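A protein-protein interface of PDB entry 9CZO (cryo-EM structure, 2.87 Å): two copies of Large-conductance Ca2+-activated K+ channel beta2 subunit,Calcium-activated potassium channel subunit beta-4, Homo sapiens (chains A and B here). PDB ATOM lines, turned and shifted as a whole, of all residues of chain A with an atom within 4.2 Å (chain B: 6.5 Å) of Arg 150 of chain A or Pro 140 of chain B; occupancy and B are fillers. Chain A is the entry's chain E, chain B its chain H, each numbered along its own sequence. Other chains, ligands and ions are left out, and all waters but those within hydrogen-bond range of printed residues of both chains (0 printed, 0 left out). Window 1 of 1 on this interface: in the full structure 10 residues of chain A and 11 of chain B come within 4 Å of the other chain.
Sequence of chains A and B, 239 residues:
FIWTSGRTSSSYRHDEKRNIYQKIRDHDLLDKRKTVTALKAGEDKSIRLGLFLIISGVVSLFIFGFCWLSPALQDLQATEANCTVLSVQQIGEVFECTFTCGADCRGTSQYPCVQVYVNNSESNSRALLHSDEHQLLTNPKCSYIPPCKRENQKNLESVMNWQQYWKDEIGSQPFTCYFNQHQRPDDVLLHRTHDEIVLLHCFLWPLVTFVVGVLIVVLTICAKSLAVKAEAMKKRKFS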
ATOM      1  N   PHE A  99      -1.993   3.808  18.181  1.00  0.00           N
ATOM      2  CA  PHE A  99      -1.444   3.604  16.835  1.00  0.00           C
ATOM      3  C   PHE A  99      -0.045   4.223  16.721  1.00  0.00           C
ATOM      4  O   PHE A  99       0.367   5.017  17.559  1.00  0.00           O
ATOM      5  CB  PHE A  99      -2.415   4.115  15.754  1.00  0.00           C
ATOM      6  CG  PHE A  99      -2.559   5.618  15.577  1.00  0.00           C
ATOM      7  CD1 PHE A  99      -1.623   6.335  14.807  1.00  0.00           C
ATOM      8  CD2 PHE A  99      -3.677   6.288  16.098  1.00  0.00           C
ATOM      9  CE1 PHE A  99      -1.782   7.714  14.595  1.00  0.00           C
ATOM     10  CE2 PHE A  99      -3.848   7.665  15.868  1.00  0.00           C
ATOM     11  CZ  PHE A  99      -2.898   8.379  15.123  1.00  0.00           C
ATOM     12  N   THR A 100       0.699   3.881  15.671  1.00  0.00           N
ATOM     13  CA  THR A 100       2.023   4.460  15.404  1.00  0.00           C
ATOM     14  C   THR A 100       2.129   5.061  14.003  1.00  0.00           C
ATOM     15  O   THR A 100       1.490   4.600  13.058  1.00  0.00           O
ATOM     16  CB  THR A 100       3.145   3.459  15.707  1.00  0.00           C
ATOM     17  OG1 THR A 100       4.390   4.117  15.637  1.00  0.00           O
ATOM     18  CG2 THR A 100       3.209   2.280  14.736  1.00  0.00           C
ATOM     19  N   CYS A 101       2.931   6.116  13.886  1.00  0.00           N
ATOM     20  CA  CYS A 101       3.166   6.902  12.675  1.00  0.00           C
ATOM     21  C   CYS A 101       4.658   7.256  12.493  1.00  0.00           C
ATOM     22  O   CYS A 101       4.994   8.210  11.790  1.00  0.00           O
ATOM     23  CB  CYS A 101       2.244   8.133  12.687  1.00  0.00           C
ATOM     24  SG  CYS A 101       2.641   9.488  13.839  1.00  0.00           S
ATOM     25  N   CYS A 105       5.590   8.246  17.839  1.00  0.00           N
ATOM     26  CA  CYS A 105       4.258   8.788  17.604  1.00  0.00           C
ATOM     27  C   CYS A 105       3.273   8.482  18.742  1.00  0.00           C
ATOM     28  O   CYS A 105       3.048   7.320  19.089  1.00  0.00           O
ATOM     29  CB  CYS A 105       3.759   8.187  16.293  1.00  0.00           C
ATOM     30  SG  CYS A 105       2.173   8.822  15.708  1.00  0.00           S
ATOM     31  N   GLY A 107       0.072   8.537  18.711  1.00  0.00           N
ATOM     32  CA  GLY A 107      -1.210   8.284  18.064  1.00  0.00           C
ATOM     33  C   GLY A 107      -2.139   7.422  18.911  1.00  0.00           C
ATOM     34  O   GLY A 107      -1.749   6.373  19.415  1.00  0.00           O
ATOM     35  N   LYS A 149      -4.887   1.121  13.954  1.00  0.00           N
ATOM     36  CA  LYS A 149      -4.442   1.889  12.799  1.00  0.00           C
ATOM     37  C   LYS A 149      -4.865   3.359  12.797  1.00  0.00           C
ATOM     38  O   LYS A 149      -5.685   3.792  13.604  1.00  0.00           O
ATOM     39  CB  LYS A 149      -4.943   1.204  11.522  1.00  0.00           C
ATOM     40  CG  LYS A 149      -4.710  -0.298  11.493  1.00  0.00           C
ATOM     41  CD  LYS A 149      -3.233  -0.639  11.595  1.00  0.00           C
ATOM     42  CE  LYS A 149      -2.407   0.149  10.590  1.00  0.00           C
ATOM     43  NZ  LYS A 149      -2.569  -0.376   9.205  1.00  0.00           N
ATOM     44  N   ARG A 150      -4.284   4.106  11.862  1.00  0.00           N
ATOM     45  CA  ARG A 150      -4.531   5.533  11.694  1.00  0.00           C
ATOM     46  C   ARG A 150      -5.997   5.945  11.526  1.00  0.00           C
ATOM     47  O   ARG A 150      -6.399   6.997  12.022  1.00  0.00           O
ATOM     48  CB  ARG A 150      -3.729   6.025  10.483  1.00  0.00           C
ATOM     49  CG  ARG A 150      -2.218   5.887  10.597  1.00  0.00           C
ATOM     50  CD  ARG A 150      -1.637   6.741  11.712  1.00  0.00           C
ATOM     51  NE  ARG A 150      -1.895   8.159  11.493  1.00  0.00           N
ATOM     52  CZ  ARG A 150      -1.166   8.934  10.698  1.00  0.00           C
ATOM     53  NH1 ARG A 150      -1.476  10.215  10.553  1.00  0.00           N
ATOM     54  NH2 ARG A 150      -0.125   8.431  10.047  1.00  0.00           N
ATOM     55  N   GLU A 151      -6.800   5.135  10.837  1.00  0.00           N
ATOM     56  CA  GLU A 151      -8.198   5.503  10.606  1.00  0.00           C
ATOM     57  C   GLU A 151      -9.218   4.637  11.387  1.00  0.00           C
ATOM     58  O   GLU A 151      -9.059   3.418  11.454  1.00  0.00           O
ATOM     59  CB  GLU A 151      -8.513   5.437   9.112  1.00  0.00           C
ATOM     60  CG  GLU A 151      -7.889   6.559   8.300  1.00  0.00           C
ATOM     61  CD  GLU A 151      -6.529   6.183   7.748  1.00  0.00           C
ATOM     62  OE1 GLU A 151      -6.002   5.119   8.139  1.00  0.00           O
ATOM     63  OE2 GLU A 151      -5.986   6.948   6.923  1.00  0.00           O
ATOM     64  N   GLN B 115      -9.141  17.120   8.573  1.00  0.00           N
ATOM     65  CA  GLN B 115      -8.224  16.292   7.799  1.00  0.00           C
ATOM     66  C   GLN B 115      -8.118  16.810   6.366  1.00  0.00           C
ATOM     67  O   GLN B 115      -9.109  17.237   5.768  1.00  0.00           O
ATOM     68  CB  GLN B 115      -8.666  14.827   7.808  1.00  0.00           C
ATOM     69  CG  GLN B 115      -8.484  14.194   9.189  1.00  0.00           C
ATOM     70  CD  GLN B 115      -8.731  12.691   9.186  1.00  0.00           C
ATOM     71  OE1 GLN B 115      -8.625  11.996  10.181  1.00  0.00           O
ATOM     72  NE2 GLN B 115      -9.053  12.127   8.044  1.00  0.00           N
ATOM     73  N   LEU B 128      -1.765  12.020   4.264  1.00  0.00           N
ATOM     74  CA  LEU B 128      -2.345  13.158   4.982  1.00  0.00           C
ATOM     75  C   LEU B 128      -1.393  14.357   4.963  1.00  0.00           C
ATOM     76  O   LEU B 128      -0.200  14.219   5.160  1.00  0.00           O
ATOM     77  CB  LEU B 128      -2.675  12.771   6.431  1.00  0.00           C
ATOM     78  CG  LEU B 128      -3.974  11.967   6.574  1.00  0.00           C
ATOM     79  CD1 LEU B 128      -4.069  11.400   7.984  1.00  0.00           C
ATOM     80  CD2 LEU B 128      -5.203  12.852   6.354  1.00  0.00           C
ATOM     81  N   HIS B 130       0.086  17.526   6.903  1.00  0.00           N
ATOM     82  CA  HIS B 130       0.336  17.749   8.332  1.00  0.00           C
ATOM     83  C   HIS B 130       1.088  19.042   8.664  1.00  0.00           C
ATOM     84  O   HIS B 130       1.325  19.338   9.824  1.00  0.00           O
ATOM     85  CB  HIS B 130       1.053  16.513   8.894  1.00  0.00           C
ATOM     86  CG  HIS B 130       0.089  15.560   9.531  1.00  0.00           C
ATOM     87  ND1 HIS B 130      -0.342  15.618  10.844  1.00  0.00           N
ATOM     88  CD2 HIS B 130      -0.555  14.555   8.912  1.00  0.00           C
ATOM     89  CE1 HIS B 130      -1.222  14.631  11.001  1.00  0.00           C
ATOM     90  NE2 HIS B 130      -1.362  13.970   9.857  1.00  0.00           N
ATOM     91  N   GLN B 135       3.493  20.123  14.773  1.00  0.00           N
ATOM     92  CA  GLN B 135       2.050  19.955  14.693  1.00  0.00           C
ATOM     93  C   GLN B 135       1.712  18.456  14.712  1.00  0.00           C
ATOM     94  O   GLN B 135       0.865  18.009  15.483  1.00  0.00           O
ATOM     95  CB  GLN B 135       1.511  20.606  13.416  1.00  0.00           C
ATOM     96  CG  GLN B 135      -0.006  20.626  13.305  1.00  0.00           C
ATOM     97  CD  GLN B 135      -0.587  19.275  12.934  1.00  0.00           C
ATOM     98  OE1 GLN B 135       0.124  18.390  12.459  1.00  0.00           O
ATOM     99  NE2 GLN B 135      -1.887  19.111  13.150  1.00  0.00           N
ATOM    100  N   LEU B 136       2.391  17.693  13.857  1.00  0.00           N
ATOM    101  CA  LEU B 136       2.158  16.257  13.749  1.00  0.00           C
ATOM    102  C   LEU B 136       2.338  15.564  15.104  1.00  0.00           C
ATOM    103  O   LEU B 136       1.468  14.815  15.541  1.00  0.00           O
ATOM    104  CB  LEU B 136       3.086  15.692  12.664  1.00  0.00           C
ATOM    105  CG  LEU B 136       2.861  14.207  12.313  1.00  0.00           C
ATOM    106  CD1 LEU B 136       3.482  13.924  10.945  1.00  0.00           C
ATOM    107  CD2 LEU B 136       3.517  13.242  13.304  1.00  0.00           C
ATOM    108  N   LEU B 137       3.436  15.827  15.810  1.00  0.00           N
ATOM    109  CA  LEU B 137       3.697  15.195  17.097  1.00  0.00           C
ATOM    110  C   LEU B 137       2.793  15.712  18.225  1.00  0.00           C
ATOM    111  O   LEU B 137       2.574  14.985  19.189  1.00  0.00           O
ATOM    112  CB  LEU B 137       5.183  15.359  17.440  1.00  0.00           C
ATOM    113  CG  LEU B 137       6.129  14.589  16.500  1.00  0.00           C
ATOM    114  CD1 LEU B 137       7.570  14.860  16.923  1.00  0.00           C
ATOM    115  CD2 LEU B 137       5.897  13.079  16.560  1.00  0.00           C
ATOM    116  N   THR B 138       2.252  16.931  18.148  1.00  0.00           N
ATOM    117  CA  THR B 138       1.316  17.442  19.168  1.00  0.00           C
ATOM    118  C   THR B 138      -0.132  17.004  18.942  1.00  0.00           C
ATOM    119  O   THR B 138      -0.855  16.826  19.919  1.00  0.00           O
ATOM    120  CB  THR B 138       1.398  18.963  19.333  1.00  0.00           C
ATOM    121  OG1 THR B 138       1.329  19.629  18.104  1.00  0.00           O
ATOM    122  CG2 THR B 138       2.692  19.382  20.020  1.00  0.00           C
ATOM    123  N   ASN B 139      -0.550  16.729  17.704  1.00  0.00           N
ATOM    124  CA  ASN B 139      -1.755  15.941  17.428  1.00  0.00           C
ATOM    125  C   ASN B 139      -1.665  15.218  16.066  1.00  0.00           C
ATOM    126  O   ASN B 139      -1.995  15.811  15.040  1.00  0.00           O
ATOM    127  CB  ASN B 139      -3.009  16.831  17.508  1.00  0.00           C
ATOM    128  CG  ASN B 139      -4.285  16.018  17.354  1.00  0.00           C
ATOM    129  OD1 ASN B 139      -4.295  14.860  17.083  1.00  0.00           O
ATOM    130  ND2 ASN B 139      -5.398  16.592  17.522  1.00  0.00           N
ATOM    131  N   PRO B 140      -1.304  13.926  16.023  1.00  0.00           N
ATOM    132  CA  PRO B 140      -1.155  13.200  14.765  1.00  0.00           C
ATOM    133  C   PRO B 140      -2.493  12.823  14.122  1.00  0.00           C
ATOM    134  O   PRO B 140      -2.505  12.330  12.997  1.00  0.00           O
ATOM    135  CB  PRO B 140      -0.323  11.962  15.109  1.00  0.00           C
ATOM    136  CG  PRO B 140      -0.703  11.697  16.557  1.00  0.00           C
ATOM    137  CD  PRO B 140      -0.890  13.097  17.138  1.00  0.00           C
ATOM    138  N   LYS B 141      -3.632  13.032  14.797  1.00  0.00           N
ATOM    139  CA  LYS B 141      -4.963  12.728  14.247  1.00  0.00           C
ATOM    140  C   LYS B 141      -5.384  13.717  13.147  1.00  0.00           C
ATOM    141  O   LYS B 141      -6.018  13.307  12.177  1.00  0.00           O
ATOM    142  CB  LYS B 141      -5.994  12.689  15.391  1.00  0.00           C
ATOM    143  CG  LYS B 141      -7.315  12.013  14.986  1.00  0.00           C
ATOM    144  CD  LYS B 141      -7.487  10.618  15.589  1.00  0.00           C
ATOM    145  CE  LYS B 141      -8.849  10.050  15.171  1.00  0.00           C
ATOM    146  NZ  LYS B 141      -9.128   8.742  15.798  1.00  0.00           N
ATOM    147  N   CYS B 142      -5.027  14.992  13.279  1.00  0.00           N
ATOM    148  CA  CYS B 142      -5.603  16.102  12.513  1.00  0.00           C
ATOM    149  C   CYS B 142      -4.545  16.905  11.738  1.00  0.00           C
ATOM    150  O   CYS B 142      -3.408  17.043  12.172  1.00  0.00           O
ATOM    151  CB  CYS B 142      -6.390  17.010  13.467  1.00  0.00           C
ATOM    152  SG  CYS B 142      -7.529  16.121  14.555  1.00  0.00           S
ATOM    153  N   SER B 143      -4.931  17.472  10.596  1.00  0.00           N
ATOM    154  CA  SER B 143      -4.040  18.161   9.650  1.00  0.00           C
ATOM    155  C   SER B 143      -3.517  19.521  10.136  1.00  0.00           C
ATOM    156  O   SER B 143      -2.477  19.994   9.680  1.00  0.00           O
ATOM    157  CB  SER B 143      -4.821  18.341   8.347  1.00  0.00           C
ATOM    158  OG  SER B 143      -4.043  18.936   7.347  1.00  0.00           O
ATOM    159  N   ASP B 186       3.017   7.977   5.058  1.00  0.00           N
ATOM    160  CA  ASP B 186       1.636   8.169   5.529  1.00  0.00           C
ATOM    161  C   ASP B 186       1.248   9.660   5.602  1.00  0.00           C
ATOM    162  O   ASP B 186       0.152  10.054   5.206  1.00  0.00           O
ATOM    163  CB  ASP B 186       1.501   7.505   6.914  1.00  0.00           C
ATOM    164  CG  ASP B 186       0.057   7.211   7.342  1.00  0.00           C
ATOM    165  OD1 ASP B 186      -0.872   7.313   6.514  1.00  0.00           O
ATOM    166  OD2 ASP B 186      -0.135   6.799   8.508  1.00  0.00           O
ATOM    167  N   ASP B 187       2.182  10.508   6.040  1.00  0.00           N
ATOM    168  CA  ASP B 187       1.989  11.943   6.246  1.00  0.00           C
ATOM    169  C   ASP B 187       2.992  12.777   5.435  1.00  0.00           C
ATOM    170  O   ASP B 187       4.122  12.352   5.208  1.00  0.00           O
ATOM    171  CB  ASP B 187       2.120  12.286   7.733  1.00  0.00           C
ATOM    172  CG  ASP B 187       1.266  11.425   8.649  1.00  0.00           C
ATOM    173  OD1 ASP B 187       0.048  11.501   8.584  1.00  0.00           O
ATOM    174  OD2 ASP B 187       1.826  10.678   9.447  1.00  0.00           O
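Cys 105 of chain A touches none of the printed residues of chain B. Arg 150 of chain A touches five residues of chain B. Of chain A, only Gly 107 (3.8 Å) and Arg 150 (3.4 Å) come within 4 Å of Pro 140 of chain B. Printed residues of chain A within 4 Å of Asp 186 of chain B: Arg 150 (2.2 Å). Of the printed residues of chain A, Asp 187 of chain B touches Arg 150. The nearest residue of chain B that does not touch Arg 150 of chain A is Lys 141 of chain B (5.0 Å). The nearest printed residue of chain B that does not touch Cys 101 of chain A is Pro 140 of chain B (4.1 Å).
The guanidinium group of Arg 150 of chain A lies within hydrogen-bond range of the backbone carbonyl oxygen of Pro 140 of chain B (3.4 Å). The guanidinium group (NE) of Arg 150 of chain A is in salt-bridge range of the side-chain carboxylate (OD2) of Asp 186 of chain B, at 3.7 Å. OD1 of Asp 187 of chain B lies within salt-bridge range of NH1 of Arg 150 of chain A, at 2.8 Å.
N of Phe 99 of chain A sits at hydrogen-bond distance from O of Gly 107 of chain A (2.9 Å). The side-chain sulfur of Cys 101 of chain A is disulfide-bonded to the side-chain sulfur of Cys 105 of chain A (2.0 Å). The side-chain sulfur (SG) of Cys 105 of chain A lies close to the backbone NH (N) of Gly 107 of chain A (3.7 Å). O of Asp 186 of chain B lies within hydrogen-bond range of N of Leu 128 of chain B, at 2.9 Å. The backbone carbonyl oxygen of His 130 of chain B lies close to the side-chain amide oxygen of Gln 135 of chain B, 3.0 Å away. A ring nitrogen (NE2) of His 130 of chain B lies within hydrogen-bond range of the side-chain carboxylate (OD1) of Asp 187 of chain B, at 3.1 Å.
Of the 8 printed residues of chain A, 3 touch a printed residue of chain B. Among the printed residues, 7 pairs touch across the chains. Among the printed residues, Asp or Glu carboxylates within 4 Å of a Lys or Arg side-chain nitrogen of the other chain: Arg 150 of chain A with Asp 186 of chain B and Arg 150 of chain A with Asp 187 of chain B.
Among the printed residues, merely in contact across the chains: Gly 107 of chain A with Pro 140 of chain B, Arg 150 of chain A with His 130 of chain B, Arg 150 of chain A with Leu 128 of chain B and Cys 101 of chain A with Leu 136 of chain B.
No position is printed for both chains. Of the 7 pairs that touch across the chains among the printed residues, none has its exchanged pair printed and touching as well.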
